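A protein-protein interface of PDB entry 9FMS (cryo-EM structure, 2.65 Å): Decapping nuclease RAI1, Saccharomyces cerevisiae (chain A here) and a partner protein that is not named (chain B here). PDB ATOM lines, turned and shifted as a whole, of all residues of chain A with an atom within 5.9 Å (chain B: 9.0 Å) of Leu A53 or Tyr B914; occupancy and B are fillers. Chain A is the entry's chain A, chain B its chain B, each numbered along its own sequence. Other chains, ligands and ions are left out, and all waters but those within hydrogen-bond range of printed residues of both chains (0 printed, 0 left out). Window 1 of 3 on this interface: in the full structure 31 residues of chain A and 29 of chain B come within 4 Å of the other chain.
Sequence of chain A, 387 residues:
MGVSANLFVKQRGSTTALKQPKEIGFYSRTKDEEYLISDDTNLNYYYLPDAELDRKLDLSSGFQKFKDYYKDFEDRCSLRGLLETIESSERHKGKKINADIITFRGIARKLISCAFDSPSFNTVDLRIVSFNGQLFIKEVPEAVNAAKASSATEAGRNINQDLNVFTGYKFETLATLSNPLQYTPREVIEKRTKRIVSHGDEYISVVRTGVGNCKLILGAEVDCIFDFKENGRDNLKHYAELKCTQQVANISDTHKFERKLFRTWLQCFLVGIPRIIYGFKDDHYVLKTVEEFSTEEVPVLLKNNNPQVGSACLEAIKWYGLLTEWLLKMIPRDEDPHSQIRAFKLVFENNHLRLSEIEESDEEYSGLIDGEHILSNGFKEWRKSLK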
ATOM      1  N   TYR A  46      21.168 -13.865   7.017  1.00  0.00           N
ATOM      2  CA  TYR A  46      22.253 -13.455   7.898  1.00  0.00           C
ATOM      3  C   TYR A  46      22.737 -14.595   8.784  1.00  0.00           C
ATOM      4  O   TYR A  46      21.916 -15.327   9.316  1.00  0.00           O
ATOM      5  CB  TYR A  46      21.782 -12.298   8.751  1.00  0.00           C
ATOM      6  CG  TYR A  46      22.885 -11.686   9.563  1.00  0.00           C
ATOM      7  CD1 TYR A  46      23.771 -10.803   8.946  1.00  0.00           C
ATOM      8  CD2 TYR A  46      23.034 -11.994  10.916  1.00  0.00           C
ATOM      9  CE1 TYR A  46      24.803 -10.220   9.682  1.00  0.00           C
ATOM     10  CE2 TYR A  46      24.067 -11.413  11.661  1.00  0.00           C
ATOM     11  CZ  TYR A  46      24.948 -10.522  11.036  1.00  0.00           C
ATOM     12  OH  TYR A  46      25.936  -9.936  11.734  1.00  0.00           O
ATOM     13  N   LEU A  48      26.305 -14.749  11.554  1.00  0.00           N
ATOM     14  CA  LEU A  48      27.648 -14.409  12.020  1.00  0.00           C
ATOM     15  C   LEU A  48      27.678 -14.389  13.549  1.00  0.00           C
ATOM     16  O   LEU A  48      27.371 -13.355  14.134  1.00  0.00           O
ATOM     17  CB  LEU A  48      28.030 -13.043  11.448  1.00  0.00           C
ATOM     18  CG  LEU A  48      29.439 -12.566  11.806  1.00  0.00           C
ATOM     19  CD1 LEU A  48      30.490 -13.317  11.017  1.00  0.00           C
ATOM     20  CD2 LEU A  48      29.602 -11.099  11.459  1.00  0.00           C
ATOM     21  N   PRO A  49      27.984 -15.509  14.210  1.00  0.00           N
ATOM     22  CA  PRO A  49      28.019 -15.606  15.660  1.00  0.00           C
ATOM     23  C   PRO A  49      29.033 -14.687  16.311  1.00  0.00           C
ATOM     24  O   PRO A  49      30.058 -14.395  15.724  1.00  0.00           O
ATOM     25  CB  PRO A  49      28.377 -17.050  15.955  1.00  0.00           C
ATOM     26  CG  PRO A  49      27.834 -17.787  14.751  1.00  0.00           C
ATOM     27  CD  PRO A  49      28.104 -16.821  13.623  1.00  0.00           C
ATOM     28  N   ASP A  50      28.828 -14.286  17.560  1.00  0.00           N
ATOM     29  CA  ASP A  50      29.754 -13.408  18.267  1.00  0.00           C
ATOM     30  C   ASP A  50      31.167 -13.989  18.386  1.00  0.00           C
ATOM     31  O   ASP A  50      32.152 -13.274  18.309  1.00  0.00           O
ATOM     32  CB  ASP A  50      29.159 -13.119  19.639  1.00  0.00           C
ATOM     33  CG  ASP A  50      30.063 -12.286  20.542  1.00  0.00           C
ATOM     34  OD1 ASP A  50      30.666 -11.303  20.073  1.00  0.00           O
ATOM     35  OD2 ASP A  50      30.174 -12.618  21.744  1.00  0.00           O
ATOM     36  N   ALA A  51      31.300 -15.305  18.503  1.00  0.00           N
ATOM     37  CA  ALA A  51      32.587 -15.984  18.539  1.00  0.00           C
ATOM     38  C   ALA A  51      33.442 -15.729  17.286  1.00  0.00           C
ATOM     39  O   ALA A  51      34.666 -15.750  17.364  1.00  0.00           O
ATOM     40  CB  ALA A  51      32.317 -17.474  18.710  1.00  0.00           C
ATOM     41  N   GLU A  52      32.849 -15.427  16.133  1.00  0.00           N
ATOM     42  CA  GLU A  52      33.596 -15.123  14.913  1.00  0.00           C
ATOM     43  C   GLU A  52      34.394 -13.835  15.020  1.00  0.00           C
ATOM     44  O   GLU A  52      35.347 -13.649  14.287  1.00  0.00           O
ATOM     45  CB  GLU A  52      32.660 -14.959  13.722  1.00  0.00           C
ATOM     46  CG  GLU A  52      31.778 -16.162  13.417  1.00  0.00           C
ATOM     47  CD  GLU A  52      32.535 -17.252  12.671  1.00  0.00           C
ATOM     48  OE1 GLU A  52      33.565 -17.733  13.183  1.00  0.00           O
ATOM     49  OE2 GLU A  52      32.078 -17.647  11.577  1.00  0.00           O
ATOM     50  N   LEU A  53      34.030 -12.930  15.913  1.00  0.00           N
ATOM     51  CA  LEU A  53      34.722 -11.663  16.070  1.00  0.00           C
ATOM     52  C   LEU A  53      36.015 -11.801  16.875  1.00  0.00           C
ATOM     53  O   LEU A  53      36.837 -10.896  16.878  1.00  0.00           O
ATOM     54  CB  LEU A  53      33.777 -10.663  16.732  1.00  0.00           C
ATOM     55  CG  LEU A  53      32.396 -10.553  16.075  1.00  0.00           C
ATOM     56  CD1 LEU A  53      31.630  -9.448  16.776  1.00  0.00           C
ATOM     57  CD2 LEU A  53      32.483 -10.246  14.590  1.00  0.00           C
ATOM     58  N   ASP A  54      36.222 -12.920  17.568  1.00  0.00           N
ATOM     59  CA  ASP A  54      37.482 -13.207  18.250  1.00  0.00           C
ATOM     60  C   ASP A  54      38.570 -13.625  17.259  1.00  0.00           C
ATOM     61  O   ASP A  54      39.747 -13.316  17.452  1.00  0.00           O
ATOM     62  CB  ASP A  54      37.287 -14.328  19.277  1.00  0.00           C
ATOM     63  CG  ASP A  54      36.310 -14.008  20.412  1.00  0.00           C
ATOM     64  OD1 ASP A  54      36.054 -12.817  20.692  1.00  0.00           O
ATOM     65  OD2 ASP A  54      35.836 -14.953  21.075  1.00  0.00           O
ATOM     66  N   ARG A  55      38.180 -14.318  16.186  1.00  0.00           N
ATOM     67  CA  ARG A  55      39.051 -14.692  15.067  1.00  0.00           C
ATOM     68  C   ARG A  55      39.406 -13.445  14.256  1.00  0.00           C
ATOM     69  O   ARG A  55      38.561 -12.588  14.029  1.00  0.00           O
ATOM     70  CB  ARG A  55      38.372 -15.738  14.167  1.00  0.00           C
ATOM     71  CG  ARG A  55      37.632 -16.848  14.925  1.00  0.00           C
ATOM     72  CD  ARG A  55      37.134 -17.940  13.974  1.00  0.00           C
ATOM     73  NE  ARG A  55      35.894 -18.571  14.458  1.00  0.00           N
ATOM     74  CZ  ARG A  55      35.719 -19.445  15.427  1.00  0.00           C
ATOM     75  NH1 ARG A  55      34.503 -19.813  15.695  1.00  0.00           N
ATOM     76  NH2 ARG A  55      36.711 -19.954  16.098  1.00  0.00           N
ATOM     77  N   LYS A  56      40.642 -13.314  13.788  1.00  0.00           N
ATOM     78  CA  LYS A  56      41.104 -12.108  13.079  1.00  0.00           C
ATOM     79  C   LYS A  56      40.731 -12.155  11.593  1.00  0.00           C
ATOM     80  O   LYS A  56      41.605 -12.236  10.738  1.00  0.00           O
ATOM     81  CB  LYS A  56      42.611 -11.903  13.328  1.00  0.00           C
ATOM     82  CG  LYS A  56      43.030 -11.898  14.810  1.00  0.00           C
ATOM     83  CD  LYS A  56      42.286 -10.851  15.648  1.00  0.00           C
ATOM     84  CE  LYS A  56      42.744 -10.831  17.110  1.00  0.00           C
ATOM     85  NZ  LYS A  56      42.360 -12.057  17.854  1.00  0.00           N
ATOM     86  N   LEU A  57      39.435 -12.169  11.273  1.00  0.00           N
ATOM     87  CA  LEU A  57      38.930 -12.276   9.898  1.00  0.00           C
ATOM     88  C   LEU A  57      39.420 -11.113   9.031  1.00  0.00           C
ATOM     89  O   LEU A  57      39.263  -9.955   9.395  1.00  0.00           O
ATOM     90  CB  LEU A  57      37.394 -12.305   9.897  1.00  0.00           C
ATOM     91  CG  LEU A  57      36.772 -13.613  10.398  1.00  0.00           C
ATOM     92  CD1 LEU A  57      35.288 -13.409  10.669  1.00  0.00           C
ATOM     93  CD2 LEU A  57      36.900 -14.725   9.361  1.00  0.00           C
ATOM     94  N   ILE A 277      23.314  -3.098  10.313  1.00  0.00           N
ATOM     95  CA  ILE A 277      24.429  -3.827  10.926  1.00  0.00           C
ATOM     96  C   ILE A 277      25.755  -3.289  10.395  1.00  0.00           C
ATOM     97  O   ILE A 277      25.990  -3.300   9.196  1.00  0.00           O
ATOM     98  CB  ILE A 277      24.251  -5.331  10.684  1.00  0.00           C
ATOM     99  CG1 ILE A 277      23.018  -5.880  11.421  1.00  0.00           C
ATOM    100  CG2 ILE A 277      25.465  -6.121  11.155  1.00  0.00           C
ATOM    101  CD1 ILE A 277      22.423  -7.110  10.755  1.00  0.00           C
ATOM    102  N   LEU A 287      38.632  -7.437  10.605  1.00  0.00           N
ATOM    103  CA  LEU A 287      37.323  -7.159  11.193  1.00  0.00           C
ATOM    104  C   LEU A 287      37.430  -7.181  12.710  1.00  0.00           C
ATOM    105  O   LEU A 287      37.612  -8.229  13.315  1.00  0.00           O
ATOM    106  CB  LEU A 287      36.324  -8.202  10.680  1.00  0.00           C
ATOM    107  CG  LEU A 287      34.917  -8.103  11.274  1.00  0.00           C
ATOM    108  CD1 LEU A 287      34.202  -6.853  10.805  1.00  0.00           C
ATOM    109  CD2 LEU A 287      34.088  -9.287  10.815  1.00  0.00           C
ATOM    110  N   LYS A 288      37.331  -6.021  13.334  1.00  0.00           N
ATOM    111  CA  LYS A 288      37.562  -5.839  14.760  1.00  0.00           C
ATOM    112  C   LYS A 288      36.335  -6.106  15.616  1.00  0.00           C
ATOM    113  O   LYS A 288      36.480  -6.674  16.688  1.00  0.00           O
ATOM    114  CB  LYS A 288      38.115  -4.425  14.987  1.00  0.00           C
ATOM    115  CG  LYS A 288      39.579  -4.437  15.412  1.00  0.00           C
ATOM    116  CD  LYS A 288      39.761  -4.969  16.840  1.00  0.00           C
ATOM    117  CE  LYS A 288      41.222  -5.161  17.251  1.00  0.00           C
ATOM    118  NZ  LYS A 288      41.933  -3.885  17.462  1.00  0.00           N
ATOM    119  N   THR A 289      35.147  -5.680  15.190  1.00  0.00           N
ATOM    120  CA  THR A 289      33.877  -5.776  15.930  1.00  0.00           C
ATOM    121  C   THR A 289      32.686  -5.675  14.980  1.00  0.00           C
ATOM    122  O   THR A 289      32.857  -5.314  13.822  1.00  0.00           O
ATOM    123  CB  THR A 289      33.718  -4.714  17.033  1.00  0.00           C
ATOM    124  OG1 THR A 289      33.163  -3.535  16.563  1.00  0.00           O
ATOM    125  CG2 THR A 289      34.981  -4.189  17.685  1.00  0.00           C
ATOM    126  N   VAL A 290      31.480  -5.985  15.444  1.00  0.00           N
ATOM    127  CA  VAL A 290      30.219  -5.724  14.742  1.00  0.00           C
ATOM    128  C   VAL A 290      29.240  -5.117  15.724  1.00  0.00           C
ATOM    129  O   VAL A 290      29.230  -5.494  16.887  1.00  0.00           O
ATOM    130  CB  VAL A 290      29.636  -6.991  14.121  1.00  0.00           C
ATOM    131  CG1 VAL A 290      28.291  -6.759  13.445  1.00  0.00           C
ATOM    132  CG2 VAL A 290      30.559  -7.558  13.059  1.00  0.00           C
ATOM    133  N   GLU A 291      28.398  -4.191  15.294  1.00  0.00           N
ATOM    134  CA  GLU A 291      27.339  -3.595  16.105  1.00  0.00           C
ATOM    135  C   GLU A 291      26.083  -3.435  15.274  1.00  0.00           C
ATOM    136  O   GLU A 291      26.138  -3.336  14.055  1.00  0.00           O
ATOM    137  CB  GLU A 291      27.751  -2.241  16.672  1.00  0.00           C
ATOM    138  CG  GLU A 291      29.015  -2.367  17.523  1.00  0.00           C
ATOM    139  CD  GLU A 291      29.422  -1.060  18.190  1.00  0.00           C
ATOM    140  OE1 GLU A 291      29.060   0.020  17.679  1.00  0.00           O
ATOM    141  OE2 GLU A 291      30.108  -1.117  19.232  1.00  0.00           O
ATOM    142  N   GLU A 292      24.932  -3.424  15.925  1.00  0.00           N
ATOM    143  CA  GLU A 292      23.648  -3.419  15.253  1.00  0.00           C
ATOM    144  C   GLU A 292      22.736  -2.341  15.814  1.00  0.00           C
ATOM    145  O   GLU A 292      22.703  -2.122  17.019  1.00  0.00           O
ATOM    146  CB  GLU A 292      23.045  -4.825  15.289  1.00  0.00           C
ATOM    147  CG  GLU A 292      22.913  -5.458  16.675  1.00  0.00           C
ATOM    148  CD  GLU A 292      22.450  -6.924  16.644  1.00  0.00           C
ATOM    149  OE1 GLU A 292      22.168  -7.450  15.547  1.00  0.00           O
ATOM    150  OE2 GLU A 292      22.328  -7.548  17.720  1.00  0.00           O
ATOM    151  N   LEU B 862      22.679 -20.630  17.135  1.00  0.00           N
ATOM    152  CA  LEU B 862      21.804 -20.068  16.107  1.00  0.00           C
ATOM    153  C   LEU B 862      21.942 -18.557  15.966  1.00  0.00           C
ATOM    154  O   LEU B 862      22.456 -17.880  16.852  1.00  0.00           O
ATOM    155  CB  LEU B 862      20.347 -20.402  16.443  1.00  0.00           C
ATOM    156  CG  LEU B 862      19.966 -21.877  16.321  1.00  0.00           C
ATOM    157  CD1 LEU B 862      18.513 -22.023  16.720  1.00  0.00           C
ATOM    158  CD2 LEU B 862      20.111 -22.416  14.908  1.00  0.00           C
ATOM    159  N   ASN B 863      21.446 -17.993  14.871  1.00  0.00           N
ATOM    160  CA  ASN B 863      21.442 -16.548  14.709  1.00  0.00           C
ATOM    161  C   ASN B 863      20.530 -15.870  15.734  1.00  0.00           C
ATOM    162  O   ASN B 863      19.415 -16.322  15.932  1.00  0.00           O
ATOM    163  CB  ASN B 863      20.990 -16.180  13.299  1.00  0.00           C
ATOM    164  CG  ASN B 863      21.120 -14.690  13.133  1.00  0.00           C
ATOM    165  OD1 ASN B 863      22.099 -14.103  13.562  1.00  0.00           O
ATOM    166  ND2 ASN B 863      20.145 -14.025  12.594  1.00  0.00           N
ATOM    167  N   GLY B 864      20.959 -14.768  16.340  1.00  0.00           N
ATOM    168  CA  GLY B 864      20.148 -13.965  17.250  1.00  0.00           C
ATOM    169  C   GLY B 864      20.105 -14.440  18.696  1.00  0.00           C
ATOM    170  O   GLY B 864      19.333 -13.906  19.478  1.00  0.00           O
ATOM    171  N   PHE B 865      20.903 -15.427  19.086  1.00  0.00           N
ATOM    172  CA  PHE B 865      21.035 -15.821  20.481  1.00  0.00           C
ATOM    173  C   PHE B 865      21.652 -14.682  21.291  1.00  0.00           C
ATOM    174  O   PHE B 865      22.738 -14.231  20.962  1.00  0.00           O
ATOM    175  CB  PHE B 865      21.864 -17.103  20.555  1.00  0.00           C
ATOM    176  CG  PHE B 865      22.506 -17.355  21.896  1.00  0.00           C
ATOM    177  CD1 PHE B 865      21.717 -17.640  23.013  1.00  0.00           C
ATOM    178  CD2 PHE B 865      23.887 -17.189  22.052  1.00  0.00           C
ATOM    179  CE1 PHE B 865      22.307 -17.693  24.282  1.00  0.00           C
ATOM    180  CE2 PHE B 865      24.482 -17.298  23.315  1.00  0.00           C
ATOM    181  CZ  PHE B 865      23.687 -17.542  24.433  1.00  0.00           C
ATOM    182  N   ILE B 866      20.993 -14.221  22.351  1.00  0.00           N
ATOM    183  CA  ILE B 866      21.514 -13.233  23.289  1.00  0.00           C
ATOM    184  C   ILE B 866      21.883 -13.967  24.575  1.00  0.00           C
ATOM    185  O   ILE B 866      21.012 -14.606  25.158  1.00  0.00           O
ATOM    186  CB  ILE B 866      20.460 -12.168  23.626  1.00  0.00           C
ATOM    187  CG1 ILE B 866      19.536 -11.682  22.507  1.00  0.00           C
ATOM    188  CG2 ILE B 866      21.127 -10.999  24.334  1.00  0.00           C
ATOM    189  CD1 ILE B 866      20.209 -10.958  21.363  1.00  0.00           C
ATOM    190  N   PRO B 867      23.109 -13.909  25.088  1.00  0.00           N
ATOM    191  CA  PRO B 867      23.452 -14.596  26.318  1.00  0.00           C
ATOM    192  C   PRO B 867      22.796 -13.956  27.537  1.00  0.00           C
ATOM    193  O   PRO B 867      22.292 -12.844  27.471  1.00  0.00           O
ATOM    194  CB  PRO B 867      24.967 -14.536  26.382  1.00  0.00           C
ATOM    195  CG  PRO B 867      25.293 -13.260  25.630  1.00  0.00           C
ATOM    196  CD  PRO B 867      24.253 -13.239  24.531  1.00  0.00           C
ATOM    197  N   LYS B 909      19.901 -11.291  28.233  1.00  0.00           N
ATOM    198  CA  LYS B 909      20.224 -10.001  28.854  1.00  0.00           C
ATOM    199  C   LYS B 909      20.612  -8.983  27.797  1.00  0.00           C
ATOM    200  O   LYS B 909      21.514  -9.217  27.002  1.00  0.00           O
ATOM    201  CB  LYS B 909      21.334 -10.204  29.880  1.00  0.00           C
ATOM    202  CG  LYS B 909      21.728  -8.916  30.611  1.00  0.00           C
ATOM    203  CD  LYS B 909      23.167  -8.509  30.296  1.00  0.00           C
ATOM    204  CE  LYS B 909      23.586  -7.332  31.176  1.00  0.00           C
ATOM    205  NZ  LYS B 909      25.019  -7.017  31.010  1.00  0.00           N
ATOM    206  N   GLY B 910      19.955  -7.835  27.796  1.00  0.00           N
ATOM    207  CA  GLY B 910      20.085  -6.864  26.720  1.00  0.00           C
ATOM    208  C   GLY B 910      19.310  -7.291  25.481  1.00  0.00           C
ATOM    209  O   GLY B 910      18.409  -8.126  25.557  1.00  0.00           O
ATOM    210  N   ILE B 911      19.630  -6.700  24.341  1.00  0.00           N
ATOM    211  CA  ILE B 911      18.867  -6.850  23.098  1.00  0.00           C
ATOM    212  C   ILE B 911      19.755  -7.031  21.868  1.00  0.00           C
ATOM    213  O   ILE B 911      19.277  -7.011  20.741  1.00  0.00           O
ATOM    214  CB  ILE B 911      17.891  -5.665  22.998  1.00  0.00           C
ATOM    215  CG1 ILE B 911      16.722  -5.953  22.059  1.00  0.00           C
ATOM    216  CG2 ILE B 911      18.595  -4.362  22.622  1.00  0.00           C
ATOM    217  CD1 ILE B 911      15.506  -5.096  22.342  1.00  0.00           C
ATOM    218  N   THR B 912      21.057  -7.212  22.071  1.00  0.00           N
ATOM    219  CA  THR B 912      22.078  -7.288  21.025  1.00  0.00           C
ATOM    220  C   THR B 912      22.894  -8.558  21.145  1.00  0.00           C
ATOM    221  O   THR B 912      23.227  -9.020  22.229  1.00  0.00           O
ATOM    222  CB  THR B 912      22.975  -6.050  21.045  1.00  0.00           C
ATOM    223  OG1 THR B 912      23.977  -6.138  20.070  1.00  0.00           O
ATOM    224  CG2 THR B 912      23.698  -5.826  22.367  1.00  0.00           C
ATOM    225  N   GLN B 913      23.198  -9.156  20.016  1.00  0.00           N
ATOM    226  CA  GLN B 913      23.845 -10.447  19.888  1.00  0.00           C
ATOM    227  C   GLN B 913      25.339 -10.419  20.232  1.00  0.00           C
ATOM    228  O   GLN B 913      25.910 -11.470  20.484  1.00  0.00           O
ATOM    229  CB  GLN B 913      23.567 -10.835  18.444  1.00  0.00           C
ATOM    230  CG  GLN B 913      24.113 -12.160  17.944  1.00  0.00           C
ATOM    231  CD  GLN B 913      23.641 -12.417  16.523  1.00  0.00           C
ATOM    232  OE1 GLN B 913      23.079 -11.580  15.853  1.00  0.00           O
ATOM    233  NE2 GLN B 913      23.828 -13.595  15.982  1.00  0.00           N
ATOM    234  N   TYR B 914      25.975  -9.245  20.274  1.00  0.00           N
ATOM    235  CA  TYR B 914      27.426  -9.050  20.344  1.00  0.00           C
ATOM    236  C   TYR B 914      27.899  -8.312  21.602  1.00  0.00           C
ATOM    237  O   TYR B 914      27.241  -7.390  22.065  1.00  0.00           O
ATOM    238  CB  TYR B 914      27.846  -8.254  19.115  1.00  0.00           C
ATOM    239  CG  TYR B 914      27.480  -8.893  17.804  1.00  0.00           C
ATOM    240  CD1 TYR B 914      28.132 -10.060  17.414  1.00  0.00           C
ATOM    241  CD2 TYR B 914      26.516  -8.322  16.971  1.00  0.00           C
ATOM    242  CE1 TYR B 914      27.802 -10.688  16.206  1.00  0.00           C
ATOM    243  CE2 TYR B 914      26.187  -8.940  15.752  1.00  0.00           C
ATOM    244  CZ  TYR B 914      26.822 -10.131  15.384  1.00  0.00           C
ATOM    245  OH  TYR B 914      26.473 -10.778  14.251  1.00  0.00           O
ATOM    246  N   LYS B 915      29.066  -8.651  22.153  1.00  0.00           N
ATOM    247  CA  LYS B 915      29.695  -7.886  23.245  1.00  0.00           C
ATOM    248  C   LYS B 915      30.204  -6.533  22.759  1.00  0.00           C
ATOM    249  O   LYS B 915      30.667  -6.458  21.627  1.00  0.00           O
ATOM    250  CB  LYS B 915      30.923  -8.610  23.792  1.00  0.00           C
ATOM    251  CG  LYS B 915      30.655  -9.974  24.404  1.00  0.00           C
ATOM    252  CD  LYS B 915      31.979 -10.565  24.906  1.00  0.00           C
ATOM    253  CE  LYS B 915      31.838 -12.050  25.226  1.00  0.00           C
ATOM    254  NZ  LYS B 915      31.798 -12.895  24.005  1.00  0.00           N
ATOM    255  N   PRO B 916      30.264  -5.487  23.590  1.00  0.00           N
ATOM    256  CA  PRO B 916      31.100  -4.336  23.321  1.00  0.00           C
ATOM    257  C   PRO B 916      32.566  -4.749  23.212  1.00  0.00           C
ATOM    258  O   PRO B 916      33.055  -5.502  24.047  1.00  0.00           O
ATOM    259  CB  PRO B 916      30.887  -3.392  24.495  1.00  0.00           C
ATOM    260  CG  PRO B 916      29.575  -3.854  25.104  1.00  0.00           C
ATOM    261  CD  PRO B 916      29.590  -5.348  24.853  1.00  0.00           C
ATOM    262  N   ARG B 917      33.286  -4.247  22.214  1.00  0.00           N
ATOM    263  CA  ARG B 917      34.715  -4.493  21.970  1.00  0.00           C
ATOM    264  C   ARG B 917      35.349  -3.202  21.490  1.00  0.00           C
ATOM    265  O   ARG B 917      34.677  -2.437  20.820  1.00  0.00           O
ATOM    266  CB  ARG B 917      34.865  -5.545  20.878  1.00  0.00           C
ATOM    267  CG  ARG B 917      34.384  -6.946  21.237  1.00  0.00           C
ATOM    268  CD  ARG B 917      34.189  -7.744  19.951  1.00  0.00           C
ATOM    269  NE  ARG B 917      33.495  -9.013  20.195  1.00  0.00           N
ATOM    270  CZ  ARG B 917      34.072 -10.134  20.531  1.00  0.00           C
ATOM    271  NH1 ARG B 917      33.411 -11.243  20.584  1.00  0.00           N
ATOM    272  NH2 ARG B 917      35.334 -10.200  20.798  1.00  0.00           N
ATOM    273  N   THR B 918      36.601  -2.910  21.804  1.00  0.00           N
ATOM    274  CA  THR B 918      37.200  -1.636  21.382  1.00  0.00           C
ATOM    275  C   THR B 918      37.308  -1.562  19.873  1.00  0.00           C
ATOM    276  O   THR B 918      37.616  -2.556  19.228  1.00  0.00           O
ATOM    277  CB  THR B 918      38.567  -1.380  22.004  1.00  0.00           C
ATOM    278  OG1 THR B 918      39.414  -2.468  21.773  1.00  0.00           O
ATOM    279  CG2 THR B 918      38.493  -1.169  23.506  1.00  0.00           C
ATOM    280  N   ARG B 922      29.287   2.230  19.353  1.00  0.00           N
ATOM    281  CA  ARG B 922      28.520   2.090  20.579  1.00  0.00           C
ATOM    282  C   ARG B 922      29.411   1.607  21.707  1.00  0.00           C
ATOM    283  O   ARG B 922      29.272   2.072  22.830  1.00  0.00           O
ATOM    284  CB  ARG B 922      27.356   1.171  20.251  1.00  0.00           C
ATOM    285  CG  ARG B 922      26.452   0.881  21.435  1.00  0.00           C
ATOM    286  CD  ARG B 922      25.138   0.299  20.907  1.00  0.00           C
ATOM    287  NE  ARG B 922      24.195   1.380  20.628  1.00  0.00           N
ATOM    288  CZ  ARG B 922      23.080   1.302  19.948  1.00  0.00           C
ATOM    289  NH1 ARG B 922      22.244   2.278  20.000  1.00  0.00           N
ATOM    290  NH2 ARG B 922      22.733   0.294  19.220  1.00  0.00           N
ATOM    291  N   ALA B 923      30.386   0.760  21.420  1.00  0.00           N
ATOM    292  CA  ALA B 923      31.399   0.370  22.384  1.00  0.00           C
ATOM    293  C   ALA B 923      32.292   1.517  22.864  1.00  0.00           C
ATOM    294  O   ALA B 923      32.721   1.487  24.012  1.00  0.00           O
ATOM    295  CB  ALA B 923      32.253  -0.719  21.760  1.00  0.00           C
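OE2 of Glu A291 is in hydrogen-bond range of N of Ala B923 (2.9 Å).
The side-chain carboxylate (OD1) of Asp A50 lies within salt-bridge range of the guanidinium group (NH1) of Arg B917, at 2.8 Å.
The side-chain amino group of Lys B915 lies within salt-bridge range of the side-chain carboxylate of Asp A50, at 2.8 Å.
The backbone NH (N) of Gln B913 lies within hydrogen-bond range of the side-chain carboxylate (OE2) of Glu A292 (2.9 Å).
The side-chain hydroxyl of Thr B912 lies within hydrogen-bond range of the side-chain carboxylate of Glu A292.
OH of Tyr B914 sits at hydrogen-bond distance from OH of Tyr A46 (2.7 Å).
OE1 of Glu A291 lies within hydrogen-bond range of N of Arg B922, at 2.8 Å.
The side-chain carboxylate (OD1) of Asp A54 is in salt-bridge range of the guanidinium group (NH2) of Arg B917 (2.7 Å).
O of Glu A292 is in hydrogen-bond range of NH2 of Arg B922, at 3.3 Å.
The backbone carbonyl oxygen (O) of Leu A48 is in hydrogen-bond range of the side-chain hydroxyl (OH) of Tyr B914 (2.7 Å).
NE2 of Gln B913 sits close to N of Gly B864.
The backbone carbonyl oxygen of Asp A54 is in hydrogen-bond range of the side-chain amino group of Lys A56, at 2.9 Å.
The side-chain amide oxygen (OD1) of Asn B863 is in hydrogen-bond range of the side-chain amide nitrogen (NE2) of Gln B913 (3.0 Å).
CD2 of Tyr A46 touches OD1 of Asn B863, at 3.5 Å.
Asp A50 touches Gln B913 (CB to O, 3.7 Å).
CA of Asp A50 touches CD1 of Tyr B914 (3.8 Å).
Tyr B914 touches Leu A53 (CD1 to CD1, 3.6 Å).
Arg B917 touches Leu A53.
Thr A289 touches Arg B917 (CG2 to CB, 3.5 Å).
Thr A289 touches Thr B918 (CG2 to O, 3.5 Å).
O of Val A290 touches CB of Tyr B914, 3.8 Å away.
Leu A53 touches two residues of chain B.
Tyr B914 touches just these residues of chain A: Tyr A46 (2.7 Å), Leu A48 (2.7 Å), Asp A50 (3.8 Å), Leu A53 (3.6 Å) and Val A290 (3.8 Å).
Of chain B, only Tyr B914 comes within 4 Å of Val A290.
Of the printed residues of chain B, Tyr A46 touches Asn B863 and Tyr B914.
Of the printed residues of chain A, Arg B917 touches Asp A50 (2.8 Å), Leu A53 (3.8 Å), Asp A54 (2.7 Å) and Thr A289 (3.5 Å).
Of the printed residues of chain A, Thr B918 touches Thr A289.
Of the printed residues of chain A, Ala B923 touches Glu A291.
The nearest residue of chain B that does not touch Leu A53 is Lys B915 (5.8 Å).
The nearest printed residue of chain A that does not touch Asn B863 is Leu A48 (4.7 Å).
Of the 18 printed residues of chain B, 9 touch a printed residue of chain A.
Hydrophobic or aromatic side chains of chain B that line the printed part of chain A: Tyr B914 and Ala B923.
Along chain A the printed residues that touch a printed residue of chain B span positions 46 to 292.
Among the printed residues, 18 pairs touch across the chains.
Among the printed residues, Asp or Glu carboxylates within 4 Å of a Lys or Arg side-chain nitrogen of the other chain: Asp A50 with Lys B915, Asp A50 with Arg B917 and Asp A54 with Arg B917.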
